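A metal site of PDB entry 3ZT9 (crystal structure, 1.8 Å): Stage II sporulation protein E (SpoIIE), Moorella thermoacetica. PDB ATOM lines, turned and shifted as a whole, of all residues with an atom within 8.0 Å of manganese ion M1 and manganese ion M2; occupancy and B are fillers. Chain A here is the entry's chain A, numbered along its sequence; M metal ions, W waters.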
ATOM      1  N   CYS A  19      10.978 -13.582 -11.147  1.00  0.00           N
ATOM      2  CA  CYS A  19       9.857 -12.938 -11.829  1.00  0.00           C
ATOM      3  C   CYS A  19       8.912 -12.291 -10.846  1.00  0.00           C
ATOM      4  O   CYS A  19       8.377 -12.942  -9.964  1.00  0.00           O
ATOM      5  CB  CYS A  19       9.111 -13.947 -12.711  1.00  0.00           C
ATOM      6  SG  CYS A  19       7.673 -13.299 -13.592  1.00  0.00           S
ATOM      7  N   GLY A  20       8.675 -10.989 -11.019  1.00  0.00           N
ATOM      8  CA  GLY A  20       7.781 -10.275 -10.104  1.00  0.00           C
ATOM      9  C   GLY A  20       6.293 -10.459 -10.320  1.00  0.00           C
ATOM     10  O   GLY A  20       5.504  -9.888  -9.580  1.00  0.00           O
ATOM     11  N   ASP A  21       5.891 -11.253 -11.310  1.00  0.00           N
ATOM     12  CA  ASP A  21       4.497 -11.618 -11.512  1.00  0.00           C
ATOM     13  C   ASP A  21       4.278 -13.067 -11.033  1.00  0.00           C
ATOM     14  O   ASP A  21       5.213 -13.845 -10.907  1.00  0.00           O
ATOM     15  CB  ASP A  21       4.091 -11.568 -13.002  1.00  0.00           C
ATOM     16  CG  ASP A  21       4.146 -10.185 -13.627  1.00  0.00           C
ATOM     17  OD1 ASP A  21       4.241  -9.162 -12.923  1.00  0.00           O
ATOM     18  OD2 ASP A  21       4.054 -10.142 -14.887  1.00  0.00           O
ATOM     19  N   GLY A  37      -1.050 -12.222 -10.667  1.00  0.00           N
ATOM     20  CA  GLY A  37      -0.703 -11.091  -9.818  1.00  0.00           C
ATOM     21  C   GLY A  37       0.560 -10.443 -10.372  1.00  0.00           C
ATOM     22  O   GLY A  37       1.397 -11.098 -11.004  1.00  0.00           O
ATOM     23  N   ASP A  38       0.711  -9.149 -10.116  1.00  0.00           N
ATOM     24  CA  ASP A  38       1.898  -8.435 -10.536  1.00  0.00           C
ATOM     25  C   ASP A  38       2.352  -7.637  -9.335  1.00  0.00           C
ATOM     26  O   ASP A  38       1.686  -6.690  -8.962  1.00  0.00           O
ATOM     27  CB  ASP A  38       1.509  -7.497 -11.722  1.00  0.00           C
ATOM     28  CG  ASP A  38       2.641  -6.572 -12.164  1.00  0.00           C
ATOM     29  OD1 ASP A  38       3.651  -6.471 -11.440  1.00  0.00           O
ATOM     30  OD2 ASP A  38       2.507  -5.918 -13.230  1.00  0.00           O
ATOM     31  N   GLY A  39       3.457  -8.024  -8.696  1.00  0.00           N
ATOM     32  CA  GLY A  39       3.961  -7.288  -7.540  1.00  0.00           C
ATOM     33  C   GLY A  39       4.513  -5.928  -7.954  1.00  0.00           C
ATOM     34  O   GLY A  39       5.177  -5.783  -8.949  1.00  0.00           O
ATOM     35  N   ILE A  40       4.288  -4.916  -7.129  1.00  0.00           N
ATOM     36  CA  ILE A  40       4.711  -3.582  -7.539  1.00  0.00           C
ATOM     37  C   ILE A  40       6.214  -3.608  -7.804  1.00  0.00           C
ATOM     38  O   ILE A  40       6.999  -4.091  -6.971  1.00  0.00           O
ATOM     39  CB  ILE A  40       4.402  -2.529  -6.472  1.00  0.00           C
ATOM     40  CG1 ILE A  40       2.893  -2.345  -6.270  1.00  0.00           C
ATOM     41  CG2 ILE A  40       5.095  -1.200  -6.850  1.00  0.00           C
ATOM     42  CD1 ILE A  40       2.215  -1.610  -7.415  1.00  0.00           C
ATOM     43  N   GLY A  41       6.623  -3.110  -8.976  1.00  0.00           N
ATOM     44  CA  GLY A  41       8.041  -3.025  -9.296  1.00  0.00           C
ATOM     45  C   GLY A  41       8.482  -4.351  -9.864  1.00  0.00           C
ATOM     46  O   GLY A  41       7.680  -5.092 -10.438  1.00  0.00           O
ATOM     47  N   HIS A  42       9.749  -4.666  -9.687  1.00  0.00           N
ATOM     48  CA  HIS A  42      10.301  -5.910 -10.214  1.00  0.00           C
ATOM     49  C   HIS A  42      11.233  -6.554  -9.193  1.00  0.00           C
ATOM     50  O   HIS A  42      11.436  -6.033  -8.100  1.00  0.00           O
ATOM     51  CB  HIS A  42      11.027  -5.688 -11.554  1.00  0.00           C
ATOM     52  CG  HIS A  42      12.025  -4.555 -11.544  1.00  0.00           C
ATOM     53  ND1 HIS A  42      13.365  -4.742 -11.265  1.00  0.00           N
ATOM     54  CD2 HIS A  42      11.873  -3.234 -11.792  1.00  0.00           C
ATOM     55  CE1 HIS A  42      13.996  -3.582 -11.337  1.00  0.00           C
ATOM     56  NE2 HIS A  42      13.114  -2.646 -11.643  1.00  0.00           N
ATOM     57  N   GLY A  43      11.772  -7.701  -9.538  1.00  0.00           N
ATOM     58  CA  GLY A  43      12.769  -8.339  -8.696  1.00  0.00           C
ATOM     59  C   GLY A  43      12.157  -9.159  -7.563  1.00  0.00           C
ATOM     60  O   GLY A  43      10.948  -9.341  -7.503  1.00  0.00           O
ATOM     61  N   ALA A  46       9.146  -7.760  -5.520  1.00  0.00           N
ATOM     62  CA  ALA A  46       7.901  -7.807  -6.254  1.00  0.00           C
ATOM     63  C   ALA A  46       7.393  -9.245  -6.317  1.00  0.00           C
ATOM     64  O   ALA A  46       6.212  -9.465  -6.185  1.00  0.00           O
ATOM     65  CB  ALA A  46       8.073  -7.244  -7.670  1.00  0.00           C
ATOM     66  N   ALA A  47       8.308 -10.190  -6.525  1.00  0.00           N
ATOM     67  CA  ALA A  47       7.939 -11.580  -6.615  1.00  0.00           C
ATOM     68  C   ALA A  47       7.314 -12.046  -5.288  1.00  0.00           C
ATOM     69  O   ALA A  47       6.312 -12.778  -5.268  1.00  0.00           O
ATOM     70  CB  ALA A  47       9.200 -12.432  -6.951  1.00  0.00           C
ATOM     71  N   ALA A  50       3.731 -10.790  -5.228  1.00  0.00           N
ATOM     72  CA  ALA A  50       2.845 -11.464  -6.191  1.00  0.00           C
ATOM     73  C   ALA A  50       2.539 -12.869  -5.686  1.00  0.00           C
ATOM     74  O   ALA A  50       1.403 -13.324  -5.761  1.00  0.00           O
ATOM     75  CB  ALA A  50       3.454 -11.523  -7.570  1.00  0.00           C
ATOM     76  N   ARG A  80       5.643  -4.960  -0.985  1.00  0.00           N
ATOM     77  CA  ARG A  80       5.633  -4.099  -2.174  1.00  0.00           C
ATOM     78  C   ARG A  80       4.210  -3.764  -2.567  1.00  0.00           C
ATOM     79  O   ARG A  80       3.968  -2.745  -3.156  1.00  0.00           O
ATOM     80  CB  ARG A  80       6.325  -4.756  -3.380  1.00  0.00           C
ATOM     81  CG  ARG A  80       7.833  -4.574  -3.414  1.00  0.00           C
ATOM     82  CD  ARG A  80       8.235  -3.188  -3.977  1.00  0.00           C
ATOM     83  NE  ARG A  80       9.703  -3.092  -4.050  1.00  0.00           N
ATOM     84  CZ  ARG A  80      10.442  -3.535  -5.054  1.00  0.00           C
ATOM     85  NH1 ARG A  80       9.879  -4.107  -6.121  1.00  0.00           N
ATOM     86  NH2 ARG A  80      11.757  -3.406  -5.011  1.00  0.00           N
ATOM     87  N   GLY A  81       3.283  -4.635  -2.223  1.00  0.00           N
ATOM     88  CA  GLY A  81       1.907  -4.532  -2.725  1.00  0.00           C
ATOM     89  C   GLY A  81       1.809  -5.215  -4.078  1.00  0.00           C
ATOM     90  O   GLY A  81       2.809  -5.534  -4.688  1.00  0.00           O
ATOM     91  N   ALA A  82       0.598  -5.438  -4.569  1.00  0.00           N
ATOM     92  CA  ALA A  82       0.449  -6.053  -5.863  1.00  0.00           C
ATOM     93  C   ALA A  82      -0.909  -5.690  -6.460  1.00  0.00           C
ATOM     94  O   ALA A  82      -1.815  -5.265  -5.744  1.00  0.00           O
ATOM     95  CB  ALA A  82       0.522  -7.578  -5.696  1.00  0.00           C
ATOM     96  N   VAL A  83      -1.032  -5.847  -7.774  1.00  0.00           N
ATOM     97  CA  VAL A  83      -2.321  -5.772  -8.447  1.00  0.00           C
ATOM     98  C   VAL A  83      -2.641  -7.213  -8.839  1.00  0.00           C
ATOM     99  O   VAL A  83      -1.723  -8.014  -8.975  1.00  0.00           O
ATOM    100  CB  VAL A  83      -2.275  -4.823  -9.672  1.00  0.00           C
ATOM    101  CG1 VAL A  83      -1.898  -3.422  -9.195  1.00  0.00           C
ATOM    102  CG2 VAL A  83      -1.281  -5.313 -10.781  1.00  0.00           C
ATOM    103  N   ASN A 103      -4.101  -3.175 -12.658  1.00  0.00           N
ATOM    104  CA  ASN A 103      -4.122  -3.177 -14.130  1.00  0.00           C
ATOM    105  C   ASN A 103      -3.775  -4.515 -14.773  1.00  0.00           C
ATOM    106  O   ASN A 103      -3.184  -4.567 -15.812  1.00  0.00           O
ATOM    107  CB  ASN A 103      -3.224  -2.098 -14.692  1.00  0.00           C
ATOM    108  CG  ASN A 103      -1.761  -2.399 -14.445  1.00  0.00           C
ATOM    109  OD1 ASN A 103      -1.424  -3.232 -13.599  1.00  0.00           O
ATOM    110  ND2 ASN A 103      -0.876  -1.733 -15.195  1.00  0.00           N
ATOM    111  N   ILE A 104      -4.163  -5.613 -14.162  1.00  0.00           N
ATOM    112  CA  ILE A 104      -4.080  -6.874 -14.850  1.00  0.00           C
ATOM    113  C   ILE A 104      -5.188  -6.872 -15.948  1.00  0.00           C
ATOM    114  O   ILE A 104      -6.254  -6.277 -15.778  1.00  0.00           O
ATOM    115  CB  ILE A 104      -4.331  -8.046 -13.873  1.00  0.00           C
ATOM    116  CG1 ILE A 104      -3.298  -8.033 -12.728  1.00  0.00           C
ATOM    117  CG2 ILE A 104      -4.328  -9.375 -14.626  1.00  0.00           C
ATOM    118  CD1 ILE A 104      -1.838  -8.278 -13.132  1.00  0.00           C
ATOM    119  N   SER A 149      -0.555  -9.897 -17.226  1.00  0.00           N
ATOM    120  CA  SER A 149      -0.078  -8.666 -16.578  1.00  0.00           C
ATOM    121  C   SER A 149       0.236  -7.605 -17.611  1.00  0.00           C
ATOM    122  O   SER A 149       0.194  -7.871 -18.827  1.00  0.00           O
ATOM    123  CB  SER A 149       1.209  -8.946 -15.808  1.00  0.00           C
ATOM    124  OG  SER A 149       2.273  -9.299 -16.681  1.00  0.00           O
ATOM    125  N   ASP A 150       0.547  -6.393 -17.143  1.00  0.00           N
ATOM    126  CA  ASP A 150       0.828  -5.286 -18.060  1.00  0.00           C
ATOM    127  C   ASP A 150       2.211  -5.436 -18.711  1.00  0.00           C
ATOM    128  O   ASP A 150       2.652  -4.529 -19.423  1.00  0.00           O
ATOM    129  CB  ASP A 150       0.695  -3.958 -17.313  1.00  0.00           C
ATOM    130  CG  ASP A 150       1.729  -3.790 -16.200  1.00  0.00           C
ATOM    131  OD1 ASP A 150       2.607  -4.663 -16.020  1.00  0.00           O
ATOM    132  OD2 ASP A 150       1.655  -2.767 -15.515  1.00  0.00           O
ATOM    133  N   GLY A 151       2.888  -6.542 -18.444  1.00  0.00           N
ATOM    134  CA  GLY A 151       4.007  -6.975 -19.294  1.00  0.00           C
ATOM    135  C   GLY A 151       3.596  -7.161 -20.743  1.00  0.00           C
ATOM    136  O   GLY A 151       4.443  -7.141 -21.652  1.00  0.00           O
ATOM    137  N   ILE A 152       2.304  -7.378 -20.986  1.00  0.00           N
ATOM    138  CA  ILE A 152       1.739  -7.354 -22.353  1.00  0.00           C
ATOM    139  C   ILE A 152       0.704  -6.217 -22.450  1.00  0.00           C
ATOM    140  O   ILE A 152      -0.160  -6.094 -21.600  1.00  0.00           O
ATOM    141  CB  ILE A 152       1.089  -8.693 -22.740  1.00  0.00           C
ATOM    142  CG1 ILE A 152       2.155  -9.793 -22.800  1.00  0.00           C
ATOM    143  CG2 ILE A 152       0.349  -8.614 -24.103  1.00  0.00           C
ATOM    144  CD1 ILE A 152       1.595 -11.178 -22.897  1.00  0.00           C
ATOM    145  N   ARG A 182       6.858  -7.460 -23.076  1.00  0.00           N
ATOM    146  CA  ARG A 182       7.944  -6.483 -23.009  1.00  0.00           C
ATOM    147  C   ARG A 182       9.144  -7.095 -22.330  1.00  0.00           C
ATOM    148  O   ARG A 182       8.995  -7.858 -21.390  1.00  0.00           O
ATOM    149  CB  ARG A 182       7.522  -5.257 -22.199  1.00  0.00           C
ATOM    150  CG  ARG A 182       6.304  -4.553 -22.741  1.00  0.00           C
ATOM    151  CD  ARG A 182       5.931  -3.428 -21.809  1.00  0.00           C
ATOM    152  NE  ARG A 182       6.998  -2.445 -21.761  1.00  0.00           N
ATOM    153  CZ  ARG A 182       6.803  -1.141 -21.593  1.00  0.00           C
ATOM    154  NH1 ARG A 182       5.577  -0.662 -21.448  1.00  0.00           N
ATOM    155  NH2 ARG A 182       7.846  -0.319 -21.583  1.00  0.00           N
ATOM    156  N   ASP A 184      11.346  -5.226 -20.749  1.00  0.00           N
ATOM    157  CA  ASP A 184      11.640  -4.350 -19.619  1.00  0.00           C
ATOM    158  C   ASP A 184      10.659  -4.492 -18.432  1.00  0.00           C
ATOM    159  O   ASP A 184      10.713  -3.738 -17.464  1.00  0.00           O
ATOM    160  CB  ASP A 184      11.784  -2.877 -20.071  1.00  0.00           C
ATOM    161  CG  ASP A 184      10.464  -2.259 -20.512  1.00  0.00           C
ATOM    162  OD1 ASP A 184       9.463  -2.969 -20.647  1.00  0.00           O
ATOM    163  OD2 ASP A 184      10.410  -1.038 -20.755  1.00  0.00           O
ATOM    164  N   ASP A 185       9.804  -5.508 -18.473  1.00  0.00           N
ATOM    165  CA  ASP A 185       8.946  -5.761 -17.327  1.00  0.00           C
ATOM    166  C   ASP A 185       8.773  -7.251 -17.254  1.00  0.00           C
ATOM    167  O   ASP A 185       9.039  -7.961 -18.242  1.00  0.00           O
ATOM    168  CB  ASP A 185       7.576  -5.065 -17.476  1.00  0.00           C
ATOM    169  CG  ASP A 185       6.799  -5.003 -16.148  1.00  0.00           C
ATOM    170  OD1 ASP A 185       7.444  -5.217 -15.086  1.00  0.00           O
ATOM    171  OD2 ASP A 185       5.582  -4.762 -16.136  1.00  0.00           O
ATOM    172  N   ASP A 186       8.343  -7.724 -16.095  1.00  0.00           N
ATOM    173  CA  ASP A 186       7.905  -9.112 -15.948  1.00  0.00           C
ATOM    174  C   ASP A 186       6.698  -9.385 -16.809  1.00  0.00           C
ATOM    175  O   ASP A 186       5.903  -8.491 -17.042  1.00  0.00           O
ATOM    176  CB  ASP A 186       7.535  -9.360 -14.504  1.00  0.00           C
ATOM    177  CG  ASP A 186       8.706  -9.103 -13.564  1.00  0.00           C
ATOM    178  OD1 ASP A 186       9.715  -9.775 -13.694  1.00  0.00           O
ATOM    179  OD2 ASP A 186       8.600  -8.233 -12.707  1.00  0.00           O
ATOM    180  N   VAL A 187       6.539 -10.629 -17.262  1.00  0.00           N
ATOM    181  CA  VAL A 187       5.399 -10.996 -18.116  1.00  0.00           C
ATOM    182  C   VAL A 187       4.717 -12.205 -17.502  1.00  0.00           C
ATOM    183  O   VAL A 187       5.383 -13.132 -17.017  1.00  0.00           O
ATOM    184  CB  VAL A 187       5.871 -11.297 -19.551  1.00  0.00           C
ATOM    185  CG1 VAL A 187       4.762 -11.965 -20.381  1.00  0.00           C
ATOM    186  CG2 VAL A 187       6.389  -9.988 -20.239  1.00  0.00           C
ATOM    187  N   ALA A 188       3.382 -12.225 -17.521  1.00  0.00           N
ATOM    188  CA  ALA A 188       2.651 -13.390 -17.075  1.00  0.00           C
ATOM    189  C   ALA A 188       1.403 -13.526 -17.934  1.00  0.00           C
ATOM    190  O   ALA A 188       0.723 -12.536 -18.185  1.00  0.00           O
ATOM    191  CB  ALA A 188       2.237 -13.243 -15.595  1.00  0.00           C
HETATM  192 MN    MN M   1       4.081  -5.092 -14.564  1.00  0.00          MN
HETATM  193 MN    MN M   2       5.601  -5.639 -11.088  1.00  0.00          MN
HETATM  194  O   HOH W   1       4.682  -3.527 -11.187  1.00  0.00           O
HETATM  195  O   HOH W   2       3.917  -3.005 -13.787  1.00  0.00           O
HETATM  196  O   HOH W   3       4.569  -7.200 -14.975  1.00  0.00           O
HETATM  197  O   HOH W   4       6.190  -7.637 -11.730  1.00  0.00           O
HETATM  198  O   HOH W   5       5.775  -4.806 -13.140  1.00  0.00           O
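C of Ile 40 touches manganese ion M2 (3.9 Å).
The nearest printed residue that does not touch manganese ion M2 is Asp 21 (4.2 Å).
O of Gly 20 is in hydrogen-bond range of N of Gly 39 (2.9 Å).
The guanidinium group (NH1) of Arg 80 lies within hydrogen-bond range of the backbone carbonyl oxygen (O) of Ile 40 (3.0 Å).
N of Ile 40 lies within hydrogen-bond range of O of Gly 81, 2.9 Å away.
The side-chain carboxylate (OD2) of Asp 150 sits at hydrogen-bond distance from the side-chain amide nitrogen (ND2) of Asn 103, 2.8 Å away.
The backbone NH (N) of Asp 38 is in hydrogen-bond range of the backbone carbonyl oxygen (O) of Val 83 (2.9 Å).
The nearest printed residue that does not touch manganese ion M1 is Gly 151 (4.3 Å).
Manganese ion M2 is bound by OD1 of Asp 38 (2.1 Å).
Water W4 binds manganese ion M2 (2.2 Å).
O of Gly 39 is bound to manganese ion M2 (2.2 Å).
Manganese ion M2 is bound by water W5, 2.2 Å away.
Manganese ion M2 is bound by the backbone carbonyl oxygen (O) of Gly 41, at 2.2 Å.
Water W1 is bound to manganese ion M2 (2.3 Å).
Manganese ion M2 has six donor atoms within binding distance.
Manganese ion M1 is bound by OD1 of Asp 150 (2.1 Å), OD2 of Asp 185 (2.2 Å), water W3 (2.2 Å), OD2 of Asp 38 (2.2 Å), water W5 (2.2 Å) and water W2 (2.2 Å).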
